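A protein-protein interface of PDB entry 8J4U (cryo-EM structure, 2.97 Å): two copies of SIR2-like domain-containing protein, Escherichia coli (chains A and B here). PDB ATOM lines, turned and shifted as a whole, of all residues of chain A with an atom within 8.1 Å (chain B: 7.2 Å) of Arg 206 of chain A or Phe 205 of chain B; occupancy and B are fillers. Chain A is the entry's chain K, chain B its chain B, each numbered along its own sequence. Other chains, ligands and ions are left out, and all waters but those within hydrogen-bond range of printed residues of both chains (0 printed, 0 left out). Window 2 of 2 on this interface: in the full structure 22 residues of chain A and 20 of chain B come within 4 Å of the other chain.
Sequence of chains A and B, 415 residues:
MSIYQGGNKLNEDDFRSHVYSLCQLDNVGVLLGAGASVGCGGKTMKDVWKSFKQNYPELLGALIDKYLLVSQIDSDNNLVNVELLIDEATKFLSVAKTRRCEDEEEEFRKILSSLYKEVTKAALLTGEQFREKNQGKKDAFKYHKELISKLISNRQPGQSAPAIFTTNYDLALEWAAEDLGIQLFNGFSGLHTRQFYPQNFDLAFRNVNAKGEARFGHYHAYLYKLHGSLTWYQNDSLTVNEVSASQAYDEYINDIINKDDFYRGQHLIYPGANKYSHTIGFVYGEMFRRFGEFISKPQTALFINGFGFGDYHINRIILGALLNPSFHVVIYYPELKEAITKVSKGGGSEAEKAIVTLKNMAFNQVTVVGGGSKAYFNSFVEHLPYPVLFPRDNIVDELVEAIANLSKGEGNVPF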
ATOM      1  N   PHE A 185      -1.015   0.292  28.710  1.00  0.00           N
ATOM      2  CA  PHE A 185       0.117   0.392  27.806  1.00  0.00           C
ATOM      3  C   PHE A 185       1.023  -0.816  27.993  1.00  0.00           C
ATOM      4  O   PHE A 185       1.416  -1.144  29.121  1.00  0.00           O
ATOM      5  CB  PHE A 185       0.874   1.700  28.027  1.00  0.00           C
ATOM      6  CG  PHE A 185       0.066   2.927  27.690  1.00  0.00           C
ATOM      7  CD1 PHE A 185      -0.848   2.905  26.649  1.00  0.00           C
ATOM      8  CD2 PHE A 185       0.221   4.098  28.408  1.00  0.00           C
ATOM      9  CE1 PHE A 185      -1.590   4.023  26.334  1.00  0.00           C
ATOM     10  CE2 PHE A 185      -0.522   5.220  28.094  1.00  0.00           C
ATOM     11  CZ  PHE A 185      -1.425   5.180  27.057  1.00  0.00           C
ATOM     12  N   SER A 189       1.816  -0.435  19.199  1.00  0.00           N
ATOM     13  CA  SER A 189       1.148   0.698  18.558  1.00  0.00           C
ATOM     14  C   SER A 189       0.769   0.320  17.135  1.00  0.00           C
ATOM     15  O   SER A 189       1.625  -0.129  16.367  1.00  0.00           O
ATOM     16  CB  SER A 189       2.055   1.922  18.560  1.00  0.00           C
ATOM     17  OG  SER A 189       2.524   2.208  19.864  1.00  0.00           O
ATOM     18  N   ASN A 200       7.814   4.130  24.620  1.00  0.00           N
ATOM     19  CA  ASN A 200       6.499   4.642  24.981  1.00  0.00           C
ATOM     20  C   ASN A 200       5.981   4.022  26.273  1.00  0.00           C
ATOM     21  O   ASN A 200       4.771   3.951  26.495  1.00  0.00           O
ATOM     22  CB  ASN A 200       5.500   4.433  23.845  1.00  0.00           C
ATOM     23  CG  ASN A 200       5.313   2.978  23.488  1.00  0.00           C
ATOM     24  OD1 ASN A 200       5.621   2.083  24.273  1.00  0.00           O
ATOM     25  ND2 ASN A 200       4.797   2.735  22.291  1.00  0.00           N
ATOM     26  N   LEU A 203       5.210   7.638  28.190  1.00  0.00           N
ATOM     27  CA  LEU A 203       4.151   8.514  27.719  1.00  0.00           C
ATOM     28  C   LEU A 203       2.985   8.529  28.700  1.00  0.00           C
ATOM     29  O   LEU A 203       2.918   7.743  29.648  1.00  0.00           O
ATOM     30  CB  LEU A 203       3.664   8.074  26.337  1.00  0.00           C
ATOM     31  CG  LEU A 203       4.579   8.333  25.139  1.00  0.00           C
ATOM     32  CD1 LEU A 203       3.932   7.815  23.873  1.00  0.00           C
ATOM     33  CD2 LEU A 203       4.905   9.801  24.997  1.00  0.00           C
ATOM     34  N   ALA A 204       2.052   9.443  28.452  1.00  0.00           N
ATOM     35  CA  ALA A 204       0.865   9.584  29.279  1.00  0.00           C
ATOM     36  C   ALA A 204      -0.165  10.392  28.507  1.00  0.00           C
ATOM     37  O   ALA A 204       0.121  10.946  27.443  1.00  0.00           O
ATOM     38  CB  ALA A 204       1.193  10.244  30.617  1.00  0.00           C
ATOM     39  N   PHE A 205      -1.372  10.451  29.056  1.00  0.00           N
ATOM     40  CA  PHE A 205      -2.473  11.176  28.445  1.00  0.00           C
ATOM     41  C   PHE A 205      -2.648  12.541  29.100  1.00  0.00           C
ATOM     42  O   PHE A 205      -2.024  12.865  30.113  1.00  0.00           O
ATOM     43  CB  PHE A 205      -3.776  10.373  28.548  1.00  0.00           C
ATOM     44  CG  PHE A 205      -4.000   9.412  27.413  1.00  0.00           C
ATOM     45  CD1 PHE A 205      -3.755   9.784  26.104  1.00  0.00           C
ATOM     46  CD2 PHE A 205      -4.478   8.138  27.658  1.00  0.00           C
ATOM     47  CE1 PHE A 205      -3.965   8.906  25.069  1.00  0.00           C
ATOM     48  CE2 PHE A 205      -4.691   7.257  26.623  1.00  0.00           C
ATOM     49  CZ  PHE A 205      -4.434   7.642  25.327  1.00  0.00           C
ATOM     50  N   ARG A 206      -3.523  13.342  28.500  1.00  0.00           N
ATOM     51  CA  ARG A 206      -3.786  14.700  28.949  1.00  0.00           C
ATOM     52  C   ARG A 206      -5.005  15.215  28.204  1.00  0.00           C
ATOM     53  O   ARG A 206      -5.201  14.888  27.031  1.00  0.00           O
ATOM     54  CB  ARG A 206      -2.573  15.606  28.703  1.00  0.00           C
ATOM     55  CG  ARG A 206      -2.911  17.035  28.340  1.00  0.00           C
ATOM     56  CD  ARG A 206      -1.677  17.913  28.354  1.00  0.00           C
ATOM     57  NE  ARG A 206      -0.927  17.805  27.106  1.00  0.00           N
ATOM     58  CZ  ARG A 206      -1.217  18.475  25.995  1.00  0.00           C
ATOM     59  NH1 ARG A 206      -2.246  19.311  25.965  1.00  0.00           N
ATOM     60  NH2 ARG A 206      -0.476  18.308  24.909  1.00  0.00           N
ATOM     61  N   ASN A 207      -5.819  16.013  28.887  1.00  0.00           N
ATOM     62  CA  ASN A 207      -7.028  16.580  28.309  1.00  0.00           C
ATOM     63  C   ASN A 207      -6.800  18.044  27.957  1.00  0.00           C
ATOM     64  O   ASN A 207      -6.018  18.743  28.607  1.00  0.00           O
ATOM     65  CB  ASN A 207      -8.214  16.452  29.268  1.00  0.00           C
ATOM     66  CG  ASN A 207      -7.888  16.931  30.664  1.00  0.00           C
ATOM     67  OD1 ASN A 207      -6.744  16.850  31.112  1.00  0.00           O
ATOM     68  ND2 ASN A 207      -8.895  17.431  31.363  1.00  0.00           N
ATOM     69  N   VAL A 208      -7.497  18.499  26.918  1.00  0.00           N
ATOM     70  CA  VAL A 208      -7.297  19.856  26.418  1.00  0.00           C
ATOM     71  C   VAL A 208      -8.113  20.855  27.228  1.00  0.00           C
ATOM     72  O   VAL A 208      -7.563  21.766  27.857  1.00  0.00           O
ATOM     73  CB  VAL A 208      -7.650  19.932  24.921  1.00  0.00           C
ATOM     74  CG1 VAL A 208      -7.156  21.240  24.328  1.00  0.00           C
ATOM     75  CG2 VAL A 208      -7.065  18.748  24.176  1.00  0.00           C
ATOM     76  N   ASN A 209      -9.436  20.704  27.217  1.00  0.00           N
ATOM     77  CA  ASN A 209     -10.333  21.647  27.872  1.00  0.00           C
ATOM     78  C   ASN A 209     -11.164  21.005  28.970  1.00  0.00           C
ATOM     79  O   ASN A 209     -11.245  21.551  30.077  1.00  0.00           O
ATOM     80  CB  ASN A 209     -11.257  22.298  26.827  1.00  0.00           C
ATOM     81  CG  ASN A 209     -12.293  21.335  26.279  1.00  0.00           C
ATOM     82  OD1 ASN A 209     -12.135  20.117  26.373  1.00  0.00           O
ATOM     83  ND2 ASN A 209     -13.362  21.876  25.709  1.00  0.00           N
ATOM     84  N   GLY A 217      -9.389  11.234  31.468  1.00  0.00           N
ATOM     85  CA  GLY A 217      -7.998  11.507  31.161  1.00  0.00           C
ATOM     86  C   GLY A 217      -7.048  10.577  31.884  1.00  0.00           C
ATOM     87  O   GLY A 217      -6.353   9.778  31.257  1.00  0.00           O
ATOM     88  N   HIS A 218      -7.021  10.677  33.212  1.00  0.00           N
ATOM     89  CA  HIS A 218      -6.130   9.849  34.014  1.00  0.00           C
ATOM     90  C   HIS A 218      -6.741   8.480  34.272  1.00  0.00           C
ATOM     91  O   HIS A 218      -6.812   8.032  35.421  1.00  0.00           O
ATOM     92  CB  HIS A 218      -5.805  10.538  35.341  1.00  0.00           C
ATOM     93  CG  HIS A 218      -5.286  11.932  35.187  1.00  0.00           C
ATOM     94  ND1 HIS A 218      -5.837  13.009  35.846  1.00  0.00           N
ATOM     95  CD2 HIS A 218      -4.262  12.425  34.452  1.00  0.00           C
ATOM     96  CE1 HIS A 218      -5.176  14.106  35.524  1.00  0.00           C
ATOM     97  NE2 HIS A 218      -4.215  13.779  34.678  1.00  0.00           N
ATOM     98  N   HIS A 220      -5.621   5.164  32.941  1.00  0.00           N
ATOM     99  CA  HIS A 220      -4.652   4.392  32.178  1.00  0.00           C
ATOM    100  C   HIS A 220      -3.612   3.833  33.135  1.00  0.00           C
ATOM    101  O   HIS A 220      -3.379   4.378  34.217  1.00  0.00           O
ATOM    102  CB  HIS A 220      -4.002   5.242  31.079  1.00  0.00           C
ATOM    103  CG  HIS A 220      -2.858   6.084  31.552  1.00  0.00           C
ATOM    104  ND1 HIS A 220      -3.018   7.118  32.448  1.00  0.00           N
ATOM    105  CD2 HIS A 220      -1.544   6.060  31.233  1.00  0.00           C
ATOM    106  CE1 HIS A 220      -1.847   7.686  32.673  1.00  0.00           C
ATOM    107  NE2 HIS A 220      -0.935   7.063  31.948  1.00  0.00           N
ATOM    108  N   GLN B 183       0.836   8.431  15.217  1.00  0.00           N
ATOM    109  CA  GLN B 183      -0.398   7.881  15.757  1.00  0.00           C
ATOM    110  C   GLN B 183      -1.530   8.866  15.505  1.00  0.00           C
ATOM    111  O   GLN B 183      -1.496   9.996  16.002  1.00  0.00           O
ATOM    112  CB  GLN B 183      -0.249   7.585  17.249  1.00  0.00           C
ATOM    113  CG  GLN B 183      -1.405   6.813  17.855  1.00  0.00           C
ATOM    114  CD  GLN B 183      -1.066   6.229  19.210  1.00  0.00           C
ATOM    115  OE1 GLN B 183       0.079   6.292  19.659  1.00  0.00           O
ATOM    116  NE2 GLN B 183      -2.064   5.653  19.870  1.00  0.00           N
ATOM    117  N   LEU B 184      -2.523   8.435  14.733  1.00  0.00           N
ATOM    118  CA  LEU B 184      -3.695   9.237  14.420  1.00  0.00           C
ATOM    119  C   LEU B 184      -4.834   8.858  15.352  1.00  0.00           C
ATOM    120  O   LEU B 184      -4.972   7.693  15.734  1.00  0.00           O
ATOM    121  CB  LEU B 184      -4.142   9.027  12.974  1.00  0.00           C
ATOM    122  CG  LEU B 184      -3.144   9.246  11.847  1.00  0.00           C
ATOM    123  CD1 LEU B 184      -3.748   8.754  10.564  1.00  0.00           C
ATOM    124  CD2 LEU B 184      -2.792  10.699  11.728  1.00  0.00           C
ATOM    125  N   PHE B 185      -5.650   9.842  15.715  1.00  0.00           N
ATOM    126  CA  PHE B 185      -6.830   9.601  16.531  1.00  0.00           C
ATOM    127  C   PHE B 185      -8.084   9.629  15.664  1.00  0.00           C
ATOM    128  O   PHE B 185      -8.297  10.572  14.891  1.00  0.00           O
ATOM    129  CB  PHE B 185      -6.921  10.621  17.661  1.00  0.00           C
ATOM    130  CG  PHE B 185      -5.776  10.549  18.631  1.00  0.00           C
ATOM    131  CD1 PHE B 185      -5.315  11.684  19.271  1.00  0.00           C
ATOM    132  CD2 PHE B 185      -5.155   9.342  18.900  1.00  0.00           C
ATOM    133  CE1 PHE B 185      -4.262  11.612  20.161  1.00  0.00           C
ATOM    134  CE2 PHE B 185      -4.105   9.267  19.786  1.00  0.00           C
ATOM    135  CZ  PHE B 185      -3.659  10.404  20.416  1.00  0.00           C
ATOM    136  N   ASP B 202     -10.837  14.416  22.608  1.00  0.00           N
ATOM    137  CA  ASP B 202     -10.431  15.478  23.519  1.00  0.00           C
ATOM    138  C   ASP B 202      -9.151  15.121  24.266  1.00  0.00           C
ATOM    139  O   ASP B 202      -8.853  15.719  25.303  1.00  0.00           O
ATOM    140  CB  ASP B 202     -11.559  15.779  24.507  1.00  0.00           C
ATOM    141  CG  ASP B 202     -12.600  16.720  23.937  1.00  0.00           C
ATOM    142  OD1 ASP B 202     -12.238  17.853  23.556  1.00  0.00           O
ATOM    143  OD2 ASP B 202     -13.782  16.326  23.867  1.00  0.00           O
ATOM    144  N   LEU B 203      -8.389  14.161  23.755  1.00  0.00           N
ATOM    145  CA  LEU B 203      -7.180  13.672  24.397  1.00  0.00           C
ATOM    146  C   LEU B 203      -5.947  14.150  23.643  1.00  0.00           C
ATOM    147  O   LEU B 203      -6.015  14.555  22.481  1.00  0.00           O
ATOM    148  CB  LEU B 203      -7.182  12.142  24.463  1.00  0.00           C
ATOM    149  CG  LEU B 203      -8.280  11.477  25.297  1.00  0.00           C
ATOM    150  CD1 LEU B 203      -8.184   9.971  25.177  1.00  0.00           C
ATOM    151  CD2 LEU B 203      -8.201  11.892  26.749  1.00  0.00           C
ATOM    152  N   ALA B 204      -4.808  14.096  24.330  1.00  0.00           N
ATOM    153  CA  ALA B 204      -3.526  14.483  23.759  1.00  0.00           C
ATOM    154  C   ALA B 204      -2.455  13.570  24.344  1.00  0.00           C
ATOM    155  O   ALA B 204      -2.757  12.559  24.983  1.00  0.00           O
ATOM    156  CB  ALA B 204      -3.246  15.967  24.025  1.00  0.00           C
ATOM    157  N   PHE B 205      -1.193  13.923  24.120  1.00  0.00           N
ATOM    158  CA  PHE B 205      -0.061  13.184  24.655  1.00  0.00           C
ATOM    159  C   PHE B 205       0.709  14.051  25.641  1.00  0.00           C
ATOM    160  O   PHE B 205       0.493  15.259  25.755  1.00  0.00           O
ATOM    161  CB  PHE B 205       0.887  12.714  23.542  1.00  0.00           C
ATOM    162  CG  PHE B 205       0.561  11.355  22.979  1.00  0.00           C
ATOM    163  CD1 PHE B 205       0.145  10.317  23.796  1.00  0.00           C
ATOM    164  CD2 PHE B 205       0.709  11.109  21.628  1.00  0.00           C
ATOM    165  CE1 PHE B 205      -0.141   9.076  23.270  1.00  0.00           C
ATOM    166  CE2 PHE B 205       0.429   9.868  21.100  1.00  0.00           C
ATOM    167  CZ  PHE B 205       0.005   8.851  21.924  1.00  0.00           C
ATOM    168  N   ARG B 206       1.619  13.402  26.363  1.00  0.00           N
ATOM    169  CA  ARG B 206       2.493  14.078  27.309  1.00  0.00           C
ATOM    170  C   ARG B 206       3.597  13.134  27.762  1.00  0.00           C
ATOM    171  O   ARG B 206       3.321  11.991  28.138  1.00  0.00           O
ATOM    172  CB  ARG B 206       1.696  14.586  28.511  1.00  0.00           C
ATOM    173  CG  ARG B 206       2.484  14.635  29.806  1.00  0.00           C
ATOM    174  CD  ARG B 206       1.743  15.391  30.887  1.00  0.00           C
ATOM    175  NE  ARG B 206       0.735  14.559  31.534  1.00  0.00           N
ATOM    176  CZ  ARG B 206       0.965  13.771  32.582  1.00  0.00           C
ATOM    177  NH1 ARG B 206       2.177  13.692  33.117  1.00  0.00           N
ATOM    178  NH2 ARG B 206      -0.026  13.054  33.094  1.00  0.00           N
ATOM    179  N   ASN B 207       4.844  13.591  27.724  1.00  0.00           N
ATOM    180  CA  ASN B 207       5.933  12.832  28.315  1.00  0.00           C
ATOM    181  C   ASN B 207       5.839  12.922  29.831  1.00  0.00           C
ATOM    182  O   ASN B 207       5.440  13.953  30.382  1.00  0.00           O
ATOM    183  CB  ASN B 207       7.285  13.352  27.828  1.00  0.00           C
ATOM    184  CG  ASN B 207       8.448  12.528  28.343  1.00  0.00           C
ATOM    185  OD1 ASN B 207       8.485  12.146  29.511  1.00  0.00           O
ATOM    186  ND2 ASN B 207       9.400  12.239  27.467  1.00  0.00           N
ATOM    187  N   GLY B 217       7.699  10.865  21.829  1.00  0.00           N
ATOM    188  CA  GLY B 217       6.743  10.439  20.826  1.00  0.00           C
ATOM    189  C   GLY B 217       5.508  11.311  20.789  1.00  0.00           C
ATOM    190  O   GLY B 217       4.423  10.845  20.445  1.00  0.00           O
ATOM    191  N   HIS B 218       5.668  12.582  21.150  1.00  0.00           N
ATOM    192  CA  HIS B 218       4.549  13.522  21.168  1.00  0.00           C
ATOM    193  C   HIS B 218       4.342  14.169  19.794  1.00  0.00           C
ATOM    194  O   HIS B 218       4.384  15.385  19.615  1.00  0.00           O
ATOM    195  CB  HIS B 218       4.752  14.553  22.274  1.00  0.00           C
ATOM    196  CG  HIS B 218       5.860  15.528  22.018  1.00  0.00           C
ATOM    197  ND1 HIS B 218       7.186  15.210  22.216  1.00  0.00           N
ATOM    198  CD2 HIS B 218       5.839  16.823  21.624  1.00  0.00           C
ATOM    199  CE1 HIS B 218       7.936  16.259  21.931  1.00  0.00           C
ATOM    200  NE2 HIS B 218       7.143  17.251  21.570  1.00  0.00           N
ATOM    201  N   TYR B 219       4.096  13.302  18.813  1.00  0.00           N
ATOM    202  CA  TYR B 219       3.495  13.660  17.536  1.00  0.00           C
ATOM    203  C   TYR B 219       2.132  12.992  17.444  1.00  0.00           C
ATOM    204  O   TYR B 219       1.965  11.849  17.882  1.00  0.00           O
ATOM    205  CB  TYR B 219       4.344  13.206  16.341  1.00  0.00           C
ATOM    206  CG  TYR B 219       5.560  14.039  16.001  1.00  0.00           C
ATOM    207  CD1 TYR B 219       5.742  15.310  16.526  1.00  0.00           C
ATOM    208  CD2 TYR B 219       6.517  13.557  15.115  1.00  0.00           C
ATOM    209  CE1 TYR B 219       6.851  16.067  16.192  1.00  0.00           C
ATOM    210  CE2 TYR B 219       7.625  14.306  14.779  1.00  0.00           C
ATOM    211  CZ  TYR B 219       7.785  15.558  15.319  1.00  0.00           C
ATOM    212  OH  TYR B 219       8.891  16.296  14.979  1.00  0.00           O
ATOM    213  N   HIS B 220       1.159  13.693  16.875  1.00  0.00           N
ATOM    214  CA  HIS B 220      -0.183  13.140  16.731  1.00  0.00           C
ATOM    215  C   HIS B 220      -0.978  14.031  15.784  1.00  0.00           C
ATOM    216  O   HIS B 220      -0.512  15.091  15.356  1.00  0.00           O
ATOM    217  CB  HIS B 220      -0.868  12.998  18.092  1.00  0.00           C
ATOM    218  CG  HIS B 220      -0.732  14.202  18.969  1.00  0.00           C
ATOM    219  ND1 HIS B 220       0.464  14.572  19.543  1.00  0.00           N
ATOM    220  CD2 HIS B 220      -1.644  15.112  19.382  1.00  0.00           C
ATOM    221  CE1 HIS B 220       0.285  15.663  20.265  1.00  0.00           C
ATOM    222  NE2 HIS B 220      -0.986  16.012  20.184  1.00  0.00           N
ATOM    223  N   TYR B 222      -5.451  14.335  14.114  1.00  0.00           N
ATOM    224  CA  TYR B 222      -6.835  13.892  14.204  1.00  0.00           C
ATOM    225  C   TYR B 222      -7.398  13.634  12.815  1.00  0.00           C
ATOM    226  O   TYR B 222      -7.144  14.401  11.881  1.00  0.00           O
ATOM    227  CB  TYR B 222      -7.683  14.924  14.938  1.00  0.00           C
ATOM    228  CG  TYR B 222      -7.346  15.047  16.403  1.00  0.00           C
ATOM    229  CD1 TYR B 222      -7.952  14.232  17.342  1.00  0.00           C
ATOM    230  CD2 TYR B 222      -6.417  15.975  16.846  1.00  0.00           C
ATOM    231  CE1 TYR B 222      -7.645  14.337  18.679  1.00  0.00           C
ATOM    232  CE2 TYR B 222      -6.103  16.087  18.181  1.00  0.00           C
ATOM    233  CZ  TYR B 222      -6.721  15.265  19.095  1.00  0.00           C
ATOM    234  OH  TYR B 222      -6.417  15.368  20.430  1.00  0.00           O
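The backbone NH (N) of Ala 204 of chain B lies within hydrogen-bond range of the backbone carbonyl oxygen (O) of Arg 206 of chain A (2.8 Å). O of Arg 206 of chain B sits at hydrogen-bond distance from N of Ala 204 of chain A (2.9 Å). The backbone NH of Val 208 of chain A lies within hydrogen-bond range of the backbone carbonyl oxygen of Asp 202 of chain B, 3.5 Å away. O of Phe 205 of chain B sits at hydrogen-bond distance from NE of Arg 206 of chain A (3.2 Å).
Among the printed residues, pairs that only touch across the chains: Leu 203 of chain A with Arg 206 of chain B, Ala 204 of chain A with Phe 205 of chain B, Phe 205 of chain A with Ala 204 of chain B, Phe 205 of chain A with Arg 206 of chain B, Arg 206 of chain A with Leu 203 of chain B, Asn 207 of chain A with Asp 202 of chain B and Asn 209 of chain A with Asp 202 of chain B.
Printed residues of chain B within 4 Å of Leu 203 of chain A: Arg 206 (3.5 Å). Of the printed residues of chain B, Phe 205 of chain A touches Ala 204 (3.2 Å) and Arg 206 (3.5 Å). Of chain B, only Leu 203 (3.5 Å), Ala 204 (2.8 Å) and Phe 205 (3.2 Å) come within 4 Å of Arg 206 of chain A. Of the printed residues of chain B, Asn 207 of chain A touches Asp 202. Printed residues of chain B within 4 Å of Val 208 of chain A: Asp 202. Gln 183 of chain B touches none of the printed residues of chain A. Leu 184 of chain B touches none of the printed residues of chain A. Printed residues of chain A within 4 Å of Leu 203 of chain B: Arg 206 (3.5 Å). Ala 204 of chain B touches just these residues of chain A: Phe 205 and Arg 206. The nearest residue of chain B that does not touch Arg 206 of chain A is Asp 202 of chain B (4.1 Å). The nearest printed residue of chain A that does not touch Leu 203 of chain B is Phe 205 of chain A (4.4 Å).
Of the 13 printed residues of chain A, 7 touch a printed residue of chain B. Hydrophobic or aromatic side chains of chain A that line the printed part of chain B: Ala 204, Phe 205 and Val 208. Of the 14 printed residues of chain B, 5 touch a printed residue of chain A. Hydrophobic or aromatic side chains of chain B within 4 Å of the printed part of chain A: Ala 204 and Phe 205. Among the printed residues, 11 pairs touch across the chains. Among the printed residues, no Asp or Glu carboxylate lies within 4 Å of a Lys or Arg side-chain nitrogen of the other chain.
Leu 203 of chain A touches Arg 206 of chain B, and with the chains exchanged Arg 206 of chain A touches Leu 203 of chain B. Ala 204 of chain A touches Phe 205 of chain B, and with the chains exchanged Phe 205 of chain A touches Ala 204 of chain B. Ala 204 of chain A touches Arg 206 of chain B, and with the chains exchanged Arg 206 of chain A touches Ala 204 of chain B. Phe 205 of chain A touches Arg 206 of chain B, and with the chains exchanged Arg 206 of chain A touches Phe 205 of chain B. 9 positions are printed for both chains. Of the 11 pairs that touch across the chains among the printed residues, 8 have their exchanged pair printed and touching as well.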
